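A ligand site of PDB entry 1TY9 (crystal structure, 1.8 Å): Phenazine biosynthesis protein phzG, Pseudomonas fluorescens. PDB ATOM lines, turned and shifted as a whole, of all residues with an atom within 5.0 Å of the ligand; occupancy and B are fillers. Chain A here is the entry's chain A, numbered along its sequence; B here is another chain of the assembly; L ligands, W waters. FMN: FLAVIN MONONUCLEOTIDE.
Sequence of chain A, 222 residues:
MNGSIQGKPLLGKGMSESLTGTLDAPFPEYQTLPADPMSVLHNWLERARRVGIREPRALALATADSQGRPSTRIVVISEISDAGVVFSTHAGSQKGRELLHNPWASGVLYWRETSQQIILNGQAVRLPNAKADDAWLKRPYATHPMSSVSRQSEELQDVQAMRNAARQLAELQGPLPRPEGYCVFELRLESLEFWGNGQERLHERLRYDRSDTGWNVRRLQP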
ATOM      1  N   GLU A  55      35.444 -17.490  25.609  1.00  0.00           N
ATOM      2  CA  GLU A  55      35.464 -18.364  24.409  1.00  0.00           C
ATOM      3  C   GLU A  55      35.838 -17.606  23.095  1.00  0.00           C
ATOM      4  O   GLU A  55      35.003 -17.548  22.155  1.00  0.00           O
ATOM      5  CB  GLU A  55      34.084 -19.016  24.220  1.00  0.00           C
ATOM      6  CG  GLU A  55      33.705 -19.913  25.371  1.00  0.00           C
ATOM      7  CD  GLU A  55      32.340 -20.550  25.249  1.00  0.00           C
ATOM      8  OE1 GLU A  55      31.915 -20.867  24.122  1.00  0.00           O
ATOM      9  OE2 GLU A  55      31.666 -20.764  26.291  1.00  0.00           O
ATOM     10  N   ALA A  58      35.536 -19.673  19.549  1.00  0.00           N
ATOM     11  CA  ALA A  58      34.219 -20.183  19.097  1.00  0.00           C
ATOM     12  C   ALA A  58      33.992 -19.605  17.674  1.00  0.00           C
ATOM     13  O   ALA A  58      33.580 -18.460  17.520  1.00  0.00           O
ATOM     14  CB  ALA A  58      33.138 -19.718  20.058  1.00  0.00           C
ATOM     15  N   THR A  72      25.710 -22.963   8.573  1.00  0.00           N
ATOM     16  CA  THR A  72      26.629 -22.459   9.615  1.00  0.00           C
ATOM     17  C   THR A  72      26.434 -23.244  10.859  1.00  0.00           C
ATOM     18  O   THR A  72      25.405 -23.922  11.014  1.00  0.00           O
ATOM     19  CB  THR A  72      26.377 -20.980   9.932  1.00  0.00           C
ATOM     20  OG1 THR A  72      24.976 -20.798  10.145  1.00  0.00           O
ATOM     21  CG2 THR A  72      26.728 -20.076   8.629  1.00  0.00           C
ATOM     22  N   ARG A  73      27.431 -23.141  11.739  1.00  0.00           N
ATOM     23  CA  ARG A  73      27.383 -23.682  13.136  1.00  0.00           C
ATOM     24  C   ARG A  73      28.656 -23.246  13.833  1.00  0.00           C
ATOM     25  O   ARG A  73      29.633 -22.858  13.173  1.00  0.00           O
ATOM     26  CB  ARG A  73      27.228 -25.218  13.167  1.00  0.00           C
ATOM     27  CG  ARG A  73      28.518 -25.965  12.782  1.00  0.00           C
ATOM     28  CD  ARG A  73      28.975 -25.720  11.292  1.00  0.00           C
ATOM     29  NE  ARG A  73      28.170 -26.476  10.334  1.00  0.00           N
ATOM     30  CZ  ARG A  73      28.142 -26.254   9.020  1.00  0.00           C
ATOM     31  NH1 ARG A  73      28.884 -25.305   8.498  1.00  0.00           N
ATOM     32  NH2 ARG A  73      27.395 -27.026   8.224  1.00  0.00           N
ATOM     33  N   ILE A  74      28.702 -23.346  15.159  1.00  0.00           N
ATOM     34  CA  ILE A  74      29.929 -23.038  15.854  1.00  0.00           C
ATOM     35  C   ILE A  74      30.801 -24.293  15.872  1.00  0.00           C
ATOM     36  O   ILE A  74      30.307 -25.398  16.193  1.00  0.00           O
ATOM     37  CB  ILE A  74      29.637 -22.611  17.301  1.00  0.00           C
ATOM     38  CG1 ILE A  74      28.689 -21.378  17.355  1.00  0.00           C
ATOM     39  CG2 ILE A  74      30.971 -22.326  18.118  1.00  0.00           C
ATOM     40  CD1 ILE A  74      29.257 -20.098  16.610  1.00  0.00           C
ATOM     41  N   VAL A  75      32.105 -24.085  15.682  1.00  0.00           N
ATOM     42  CA  VAL A  75      33.137 -25.101  16.006  1.00  0.00           C
ATOM     43  C   VAL A  75      34.240 -24.376  16.760  1.00  0.00           C
ATOM     44  O   VAL A  75      34.335 -23.115  16.675  1.00  0.00           O
ATOM     45  CB  VAL A  75      33.741 -25.904  14.743  1.00  0.00           C
ATOM     46  CG1 VAL A  75      32.602 -26.625  13.912  1.00  0.00           C
ATOM     47  CG2 VAL A  75      34.587 -24.937  13.757  1.00  0.00           C
ATOM     48  N   VAL A  76      35.061 -25.139  17.487  1.00  0.00           N
ATOM     49  CA  VAL A  76      36.190 -24.552  18.278  1.00  0.00           C
ATOM     50  C   VAL A  76      37.502 -24.696  17.483  1.00  0.00           C
ATOM     51  O   VAL A  76      37.872 -25.802  17.038  1.00  0.00           O
ATOM     52  CB  VAL A  76      36.351 -25.232  19.647  1.00  0.00           C
ATOM     53  CG1 VAL A  76      37.618 -24.704  20.443  1.00  0.00           C
ATOM     54  CG2 VAL A  76      35.031 -25.071  20.429  1.00  0.00           C
ATOM     55  N   SER A  88      38.192 -29.920  14.772  1.00  0.00           N
ATOM     56  CA  SER A  88      37.836 -31.343  14.654  1.00  0.00           C
ATOM     57  C   SER A  88      36.302 -31.448  14.550  1.00  0.00           C
ATOM     58  O   SER A  88      35.589 -30.612  15.053  1.00  0.00           O
ATOM     59  CB  SER A  88      38.281 -32.097  15.930  1.00  0.00           C
ATOM     60  OG  SER A  88      39.683 -32.325  15.903  1.00  0.00           O
ATOM     61  N   THR A  89      35.792 -32.491  13.893  1.00  0.00           N
ATOM     62  CA  THR A  89      34.359 -32.688  13.731  1.00  0.00           C
ATOM     63  C   THR A  89      34.119 -34.126  13.313  1.00  0.00           C
ATOM     64  O   THR A  89      35.032 -34.955  13.410  1.00  0.00           O
ATOM     65  CB  THR A  89      33.761 -31.682  12.667  1.00  0.00           C
ATOM     66  OG1 THR A  89      32.322 -31.784  12.640  1.00  0.00           O
ATOM     67  CG2 THR A  89      34.231 -32.050  11.203  1.00  0.00           C
ATOM     68  N   HIS A  90      32.900 -34.439  12.858  1.00  0.00           N
ATOM     69  CA  HIS A  90      32.669 -35.771  12.298  1.00  0.00           C
ATOM     70  C   HIS A  90      32.495 -35.723  10.790  1.00  0.00           C
ATOM     71  O   HIS A  90      31.796 -34.868  10.262  1.00  0.00           O
ATOM     72  CB  HIS A  90      31.480 -36.465  12.968  1.00  0.00           C
ATOM     73  CG  HIS A  90      31.745 -36.716  14.407  1.00  0.00           C
ATOM     74  ND1 HIS A  90      32.098 -37.963  14.899  1.00  0.00           N
ATOM     75  CD2 HIS A  90      31.855 -35.854  15.457  1.00  0.00           C
ATOM     76  CE1 HIS A  90      32.380 -37.856  16.185  1.00  0.00           C
ATOM     77  NE2 HIS A  90      32.211 -36.589  16.546  1.00  0.00           N
ATOM     78  N   SER A  93      28.879 -35.642   9.342  1.00  0.00           N
ATOM     79  CA  SER A  93      27.983 -34.461   9.712  1.00  0.00           C
ATOM     80  C   SER A  93      27.640 -33.651   8.484  1.00  0.00           C
ATOM     81  O   SER A  93      28.245 -33.832   7.382  1.00  0.00           O
ATOM     82  CB  SER A  93      28.659 -33.518  10.747  1.00  0.00           C
ATOM     83  OG  SER A  93      29.862 -32.956  10.208  1.00  0.00           O
ATOM     84  N   GLN A  94      26.722 -32.714   8.634  1.00  0.00           N
ATOM     85  CA  GLN A  94      26.463 -31.843   7.464  1.00  0.00           C
ATOM     86  C   GLN A  94      27.751 -31.117   7.030  1.00  0.00           C
ATOM     87  O   GLN A  94      27.970 -30.939   5.829  1.00  0.00           O
ATOM     88  CB  GLN A  94      25.343 -30.846   7.771  1.00  0.00           C
ATOM     89  CG  GLN A  94      25.085 -29.853   6.639  1.00  0.00           C
ATOM     90  CD  GLN A  94      23.746 -29.141   6.787  1.00  0.00           C
ATOM     91  OE1 GLN A  94      22.921 -29.490   7.652  1.00  0.00           O
ATOM     92  NE2 GLN A  94      23.499 -28.202   5.906  1.00  0.00           N
ATOM     93  N   LYS A  95      28.583 -30.619   7.962  1.00  0.00           N
ATOM     94  CA  LYS A  95      29.688 -29.736   7.489  1.00  0.00           C
ATOM     95  C   LYS A  95      30.715 -30.656   6.788  1.00  0.00           C
ATOM     96  O   LYS A  95      31.405 -30.250   5.856  1.00  0.00           O
ATOM     97  CB  LYS A  95      30.358 -28.943   8.634  1.00  0.00           C
ATOM     98  CG  LYS A  95      31.393 -29.749   9.529  1.00  0.00           C
ATOM     99  CD  LYS A  95      31.645 -29.025  10.853  1.00  0.00           C
ATOM    100  CE  LYS A  95      30.405 -29.026  11.863  1.00  0.00           C
ATOM    101  NZ  LYS A  95      29.989 -30.419  12.142  1.00  0.00           N
ATOM    102  N   GLY A  96      30.816 -31.892   7.243  1.00  0.00           N
ATOM    103  CA  GLY A  96      31.805 -32.809   6.682  1.00  0.00           C
ATOM    104  C   GLY A  96      31.444 -33.280   5.304  1.00  0.00           C
ATOM    105  O   GLY A  96      32.302 -33.312   4.404  1.00  0.00           O
ATOM    106  N   GLN A 152      26.828 -37.889  14.112  1.00  0.00           N
ATOM    107  CA  GLN A 152      26.507 -36.495  14.198  1.00  0.00           C
ATOM    108  C   GLN A 152      25.667 -36.044  12.997  1.00  0.00           C
ATOM    109  O   GLN A 152      26.053 -36.222  11.845  1.00  0.00           O
ATOM    110  CB  GLN A 152      27.822 -35.680  14.273  1.00  0.00           C
ATOM    111  CG  GLN A 152      27.619 -34.167  14.519  1.00  0.00           C
ATOM    112  CD  GLN A 152      28.950 -33.439  14.785  1.00  0.00           C
ATOM    113  OE1 GLN A 152      29.218 -33.004  15.920  1.00  0.00           O
ATOM    114  NE2 GLN A 152      29.808 -33.363  13.775  1.00  0.00           N
ATOM    115  N   SER A 153      24.537 -35.415  13.351  1.00  0.00           N
ATOM    116  CA  SER A 153      23.620 -34.694  12.446  1.00  0.00           C
ATOM    117  C   SER A 153      22.651 -35.607  11.724  1.00  0.00           C
ATOM    118  O   SER A 153      21.750 -35.132  11.076  1.00  0.00           O
ATOM    119  CB  SER A 153      24.365 -33.689  11.516  1.00  0.00           C
ATOM    120  OG  SER A 153      25.363 -32.963  12.285  1.00  0.00           O
ATOM    121  N   LEU B  19      32.899 -25.528  26.921  1.00  0.00           N
ATOM    122  CA  LEU B  19      31.914 -24.451  26.926  1.00  0.00           C
ATOM    123  C   LEU B  19      31.863 -23.839  28.332  1.00  0.00           C
ATOM    124  O   LEU B  19      32.059 -24.549  29.326  1.00  0.00           O
ATOM    125  CB  LEU B  19      30.514 -24.971  26.576  1.00  0.00           C
ATOM    126  CG  LEU B  19      30.381 -25.740  25.264  1.00  0.00           C
ATOM    127  CD1 LEU B  19      29.056 -25.496  24.679  1.00  0.00           C
ATOM    128  CD2 LEU B  19      31.411 -25.308  24.312  1.00  0.00           C
ATOM    129  N   TYR B 110      24.960 -17.439  18.724  1.00  0.00           N
ATOM    130  CA  TYR B 110      25.528 -18.259  19.764  1.00  0.00           C
ATOM    131  C   TYR B 110      25.635 -17.440  21.063  1.00  0.00           C
ATOM    132  O   TYR B 110      26.274 -16.334  21.125  1.00  0.00           O
ATOM    133  CB  TYR B 110      26.902 -18.925  19.351  1.00  0.00           C
ATOM    134  CG  TYR B 110      27.612 -19.589  20.539  1.00  0.00           C
ATOM    135  CD1 TYR B 110      26.969 -20.551  21.290  1.00  0.00           C
ATOM    136  CD2 TYR B 110      28.965 -19.225  20.897  1.00  0.00           C
ATOM    137  CE1 TYR B 110      27.597 -21.123  22.370  1.00  0.00           C
ATOM    138  CE2 TYR B 110      29.593 -19.797  21.977  1.00  0.00           C
ATOM    139  CZ  TYR B 110      28.874 -20.733  22.728  1.00  0.00           C
ATOM    140  OH  TYR B 110      29.466 -21.307  23.771  1.00  0.00           O
ATOM    141  N   GLN B 117      22.668 -22.289  20.761  1.00  0.00           N
ATOM    142  CA  GLN B 117      22.919 -21.800  19.398  1.00  0.00           C
ATOM    143  C   GLN B 117      21.636 -21.852  18.582  1.00  0.00           C
ATOM    144  O   GLN B 117      20.787 -22.696  18.804  1.00  0.00           O
ATOM    145  CB  GLN B 117      24.115 -22.576  18.844  1.00  0.00           C
ATOM    146  CG  GLN B 117      24.043 -23.248  17.598  1.00  0.00           C
ATOM    147  CD  GLN B 117      25.344 -24.042  17.343  1.00  0.00           C
ATOM    148  OE1 GLN B 117      25.461 -25.294  17.622  1.00  0.00           O
ATOM    149  NE2 GLN B 117      26.291 -23.357  16.780  1.00  0.00           N
ATOM    150  N   GLU B 193      17.614 -24.666  13.211  1.00  0.00           N
ATOM    151  CA  GLU B 193      17.936 -25.605  14.299  1.00  0.00           C
ATOM    152  C   GLU B 193      18.086 -24.790  15.590  1.00  0.00           C
ATOM    153  O   GLU B 193      18.705 -23.732  15.582  1.00  0.00           O
ATOM    154  CB  GLU B 193      19.227 -26.428  14.050  1.00  0.00           C
ATOM    155  CG  GLU B 193      19.717 -27.196  15.298  1.00  0.00           C
ATOM    156  CD  GLU B 193      20.995 -27.954  15.050  1.00  0.00           C
ATOM    157  OE1 GLU B 193      21.312 -28.208  13.857  1.00  0.00           O
ATOM    158  OE2 GLU B 193      21.680 -28.252  16.014  1.00  0.00           O
ATOM    159  N   TRP B 195      19.798 -25.447  19.239  1.00  0.00           N
ATOM    160  CA  TRP B 195      20.804 -26.283  19.803  1.00  0.00           C
ATOM    161  C   TRP B 195      21.005 -25.883  21.307  1.00  0.00           C
ATOM    162  O   TRP B 195      21.288 -24.721  21.602  1.00  0.00           O
ATOM    163  CB  TRP B 195      22.110 -26.086  18.975  1.00  0.00           C
ATOM    164  CG  TRP B 195      23.257 -27.001  19.412  1.00  0.00           C
ATOM    165  CD1 TRP B 195      23.769 -28.053  18.682  1.00  0.00           C
ATOM    166  CD2 TRP B 195      24.086 -26.897  20.602  1.00  0.00           C
ATOM    167  NE1 TRP B 195      24.834 -28.620  19.340  1.00  0.00           N
ATOM    168  CE2 TRP B 195      25.058 -27.916  20.524  1.00  0.00           C
ATOM    169  CE3 TRP B 195      24.119 -26.023  21.697  1.00  0.00           C
ATOM    170  CZ2 TRP B 195      25.986 -28.135  21.532  1.00  0.00           C
ATOM    171  CZ3 TRP B 195      25.073 -26.232  22.680  1.00  0.00           C
ATOM    172  CH2 TRP B 195      25.963 -27.276  22.608  1.00  0.00           C
ATOM    173  N   ARG B 205      19.278 -31.033  19.853  1.00  0.00           N
ATOM    174  CA  ARG B 205      19.217 -30.443  18.541  1.00  0.00           C
ATOM    175  C   ARG B 205      17.836 -30.566  17.944  1.00  0.00           C
ATOM    176  O   ARG B 205      17.385 -31.660  17.633  1.00  0.00           O
ATOM    177  CB  ARG B 205      20.219 -31.080  17.625  1.00  0.00           C
ATOM    178  CG  ARG B 205      21.692 -31.019  18.130  1.00  0.00           C
ATOM    179  CD  ARG B 205      22.691 -31.558  17.132  1.00  0.00           C
ATOM    180  NE  ARG B 205      22.830 -30.776  15.902  1.00  0.00           N
ATOM    181  CZ  ARG B 205      23.467 -31.179  14.814  1.00  0.00           C
ATOM    182  NH1 ARG B 205      24.105 -32.357  14.804  1.00  0.00           N
ATOM    183  NH2 ARG B 205      23.494 -30.364  13.736  1.00  0.00           N
ATOM    184  N   PRO B 222      23.854 -35.463  18.198  1.00  0.00           N
ATOM    185  CA  PRO B 222      24.843 -34.456  18.610  1.00  0.00           C
ATOM    186  C   PRO B 222      26.194 -34.654  17.904  1.00  0.00           C
ATOM    187  O   PRO B 222      26.894 -33.699  17.699  1.00  0.00           O
ATOM    188  CB  PRO B 222      24.960 -34.670  20.124  1.00  0.00           C
ATOM    189  CG  PRO B 222      24.444 -36.011  20.415  1.00  0.00           C
ATOM    190  CD  PRO B 222      23.517 -36.427  19.265  1.00  0.00           C
ATOM    191  OXT PRO B 222      26.639 -35.762  17.550  1.00  0.00           O
HETATM  192  N1  FMN L   1      30.903 -29.570  16.735  1.00  0.00           N
HETATM  193  C2  FMN L   1      32.059 -30.136  16.244  1.00  0.00           C
HETATM  194  O2  FMN L   1      31.959 -31.055  15.521  1.00  0.00           O
HETATM  195  N3  FMN L   1      33.294 -29.635  16.578  1.00  0.00           N
HETATM  196  C4  FMN L   1      33.483 -28.564  17.400  1.00  0.00           C
HETATM  197  O4  FMN L   1      34.651 -28.085  17.504  1.00  0.00           O
HETATM  198  C4A FMN L   1      32.348 -27.992  17.993  1.00  0.00           C
HETATM  199  N5  FMN L   1      32.427 -26.940  18.864  1.00  0.00           N
HETATM  200  C5A FMN L   1      31.262 -26.406  19.324  1.00  0.00           C
HETATM  201  C6  FMN L   1      31.367 -25.331  20.202  1.00  0.00           C
HETATM  202  C7  FMN L   1      30.235 -24.746  20.689  1.00  0.00           C
HETATM  203  C7M FMN L   1      30.490 -23.536  21.575  1.00  0.00           C
HETATM  204  C8  FMN L   1      28.964 -25.236  20.351  1.00  0.00           C
HETATM  205  C8M FMN L   1      27.688 -24.498  20.660  1.00  0.00           C
HETATM  206  C9  FMN L   1      28.828 -26.304  19.461  1.00  0.00           C
HETATM  207  C9A FMN L   1      29.995 -26.909  18.981  1.00  0.00           C
HETATM  208  N10 FMN L   1      29.895 -27.994  18.136  1.00  0.00           N
HETATM  209  C10 FMN L   1      31.052 -28.481  17.599  1.00  0.00           C
HETATM  210  C1' FMN L   1      28.592 -28.458  17.610  1.00  0.00           C
HETATM  211  C2' FMN L   1      28.311 -27.836  16.183  1.00  0.00           C
HETATM  212  O2' FMN L   1      27.811 -26.479  16.341  1.00  0.00           O
HETATM  213  C3' FMN L   1      27.241 -28.613  15.410  1.00  0.00           C
HETATM  214  O3' FMN L   1      26.146 -28.869  16.281  1.00  0.00           O
HETATM  215  C4' FMN L   1      27.772 -29.973  14.914  1.00  0.00           C
HETATM  216  O4' FMN L   1      29.151 -29.866  14.613  1.00  0.00           O
HETATM  217  C5' FMN L   1      26.944 -30.400  13.722  1.00  0.00           C
HETATM  218  O5' FMN L   1      27.031 -29.360  12.732  1.00  0.00           O
HETATM  219  P   FMN L   1      26.508 -29.747  11.245  1.00  0.00           P
HETATM  220  O1P FMN L   1      26.199 -28.404  10.729  1.00  0.00           O
HETATM  221  O2P FMN L   1      27.606 -30.409  10.470  1.00  0.00           O
HETATM  222  O3P FMN L   1      25.219 -30.557  11.379  1.00  0.00           O
HETATM  223  O   HOH W   1      33.253 -33.138  17.398  1.00  0.00           O
HETATM  224  O   HOH W   2      22.840 -30.152  10.200  1.00  0.00           O
HETATM  225  O   HOH W   3      24.251 -26.081   9.766  1.00  0.00           O
HETATM  226  O   HOH W   4      37.313 -28.378  17.129  1.00  0.00           O
HETATM  227  O   HOH W   5      24.353 -27.252  12.632  1.00  0.00           O
HETATM  228  O   HOH W   6      25.969 -30.867  18.416  1.00  0.00           O
HETATM  229  O   HOH W   7      24.307 -27.368  15.346  1.00  0.00           O
HETATM  230  O   HOH W   8      30.235 -30.542  20.116  1.00  0.00           O
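An oxygen (O3P) of the ligand lies within hydrogen-bond range of the side-chain hydroxyl (OG) of Ser 153 (2.6 Å). The backbone NH of Lys 95 sits at hydrogen-bond distance from an oxygen (O2P) of the ligand, at 2.7 Å. The side-chain amino group (NZ) of Lys 95 lies within salt-bridge range of an oxygen (O2P) of the ligand (2.9 Å). An oxygen (O2') of the ligand lies within hydrogen-bond range of the backbone NH (N) of Ile 74 (3.5 Å). O2' of the ligand sits at hydrogen-bond distance from O of Ile 74 (2.7 Å). NE of Arg 73 is in salt-bridge range of O1P of the ligand (2.8 Å). O of Ser 88 is in hydrogen-bond range of N3 of the ligand (2.9 Å). The side-chain amide oxygen (OE1) of Gln 117 of chain B is in hydrogen-bond range of an oxygen (O2') of the ligand (2.9 Å). O3P of the ligand is in salt-bridge range of NH2 of Arg 205 of chain B (2.9 Å). An oxygen (O4) of the ligand lies within hydrogen-bond range of the backbone NH (N) of Val 76 (3.0 Å). The side-chain hydroxyl (OG1) of Thr 89 sits at hydrogen-bond distance from an oxygen (O2) of the ligand. An oxygen (O2P) of the ligand is in hydrogen-bond range of the backbone NH (N) of Gln 94. The side-chain hydroxyl (OG) of Ser 93 sits close to an oxygen (O2P) of the ligand, at 3.4 Å. The indole nitrogen (NE1) of Trp 195 of chain B sits at hydrogen-bond distance from an oxygen (O3') of the ligand (3.3 Å). The side-chain amide oxygen (OE1) of Gln 152 sits close to an oxygen (O2) of the ligand, at 3.4 Å.
The side-chain hydroxyl (OG) of Ser 153 sits at hydrogen-bond distance from the guanidinium group (NH1) of Arg 205 of chain B, 2.9 Å away. The side-chain amino group (NZ) of Lys 95 is in hydrogen-bond range of the side-chain hydroxyl (OG1) of Thr 89 (2.7 Å). N of Ile 74 sits close to NE2 of Gln 117 of chain B (2.9 Å). The backbone NH of Gln 117 of chain B sits at hydrogen-bond distance from the backbone carbonyl oxygen of Trp 195 of chain B, at 2.9 Å. OE2 of Glu 193 of chain B is in salt-bridge range of NE of Arg 205 of chain B (2.8 Å). The side-chain amide nitrogen of Gln 152 lies within hydrogen-bond range of the side-chain hydroxyl of Thr 89 (3.2 Å). The side-chain hydroxyl (OG) of Ser 93 is in hydrogen-bond range of the backbone NH (N) of Gly 96 (3.3 Å). The backbone NH (N) of His 90 sits close to the side-chain amide nitrogen (NE2) of Gln 152.
Water W7 lies within hydrogen-bond range of O3' of the ligand (2.6 Å), OE2 of Glu 193 of chain B (2.9 Å), OE1 of Gln 117 of chain B (3.3 Å) and NH2 of Arg 205 of chain B (3.5 Å). Water W2 bridges OE1 of Gln 94 (2.6 Å) and O3P of the ligand (2.7 Å). Water W4 lies within hydrogen-bond range of O of Val 76, O4 of the ligand and N of Ser 88. Water W5 lies within hydrogen-bond range of an oxygen (O1P) of the ligand, the guanidinium group of Arg 205 of chain B and the side-chain carboxylate of Glu 193 of chain B. Water W6 lies within hydrogen-bond range of NE1 of Trp 195 of chain B, O3' of the ligand and O of Pro 222 of chain B. Water W3 lies within hydrogen-bond range of the backbone carbonyl oxygen (O) of Thr 72 (2.7 Å) and an oxygen (O1P) of the ligand (3.2 Å).
Glu 55 touches the ligand. Val 75 touches the ligand (CA to N5, 3.5 Å). Leu 19 of chain B touches the ligand (CD2 to C7M, 3.4 Å). Tyr 110 of chain B touches the ligand. Within 4 Å of the ligand: Glu 55, Arg 73, Ile 74, Val 75, Val 76, Ser 88, Thr 89, Ser 93, Gln 94, Lys 95, Gln 152, Ser 153, Leu 19 of chain B, Tyr 110 of chain B, Gln 117 of chain B, Trp 195 of chain B and Arg 205 of chain B.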
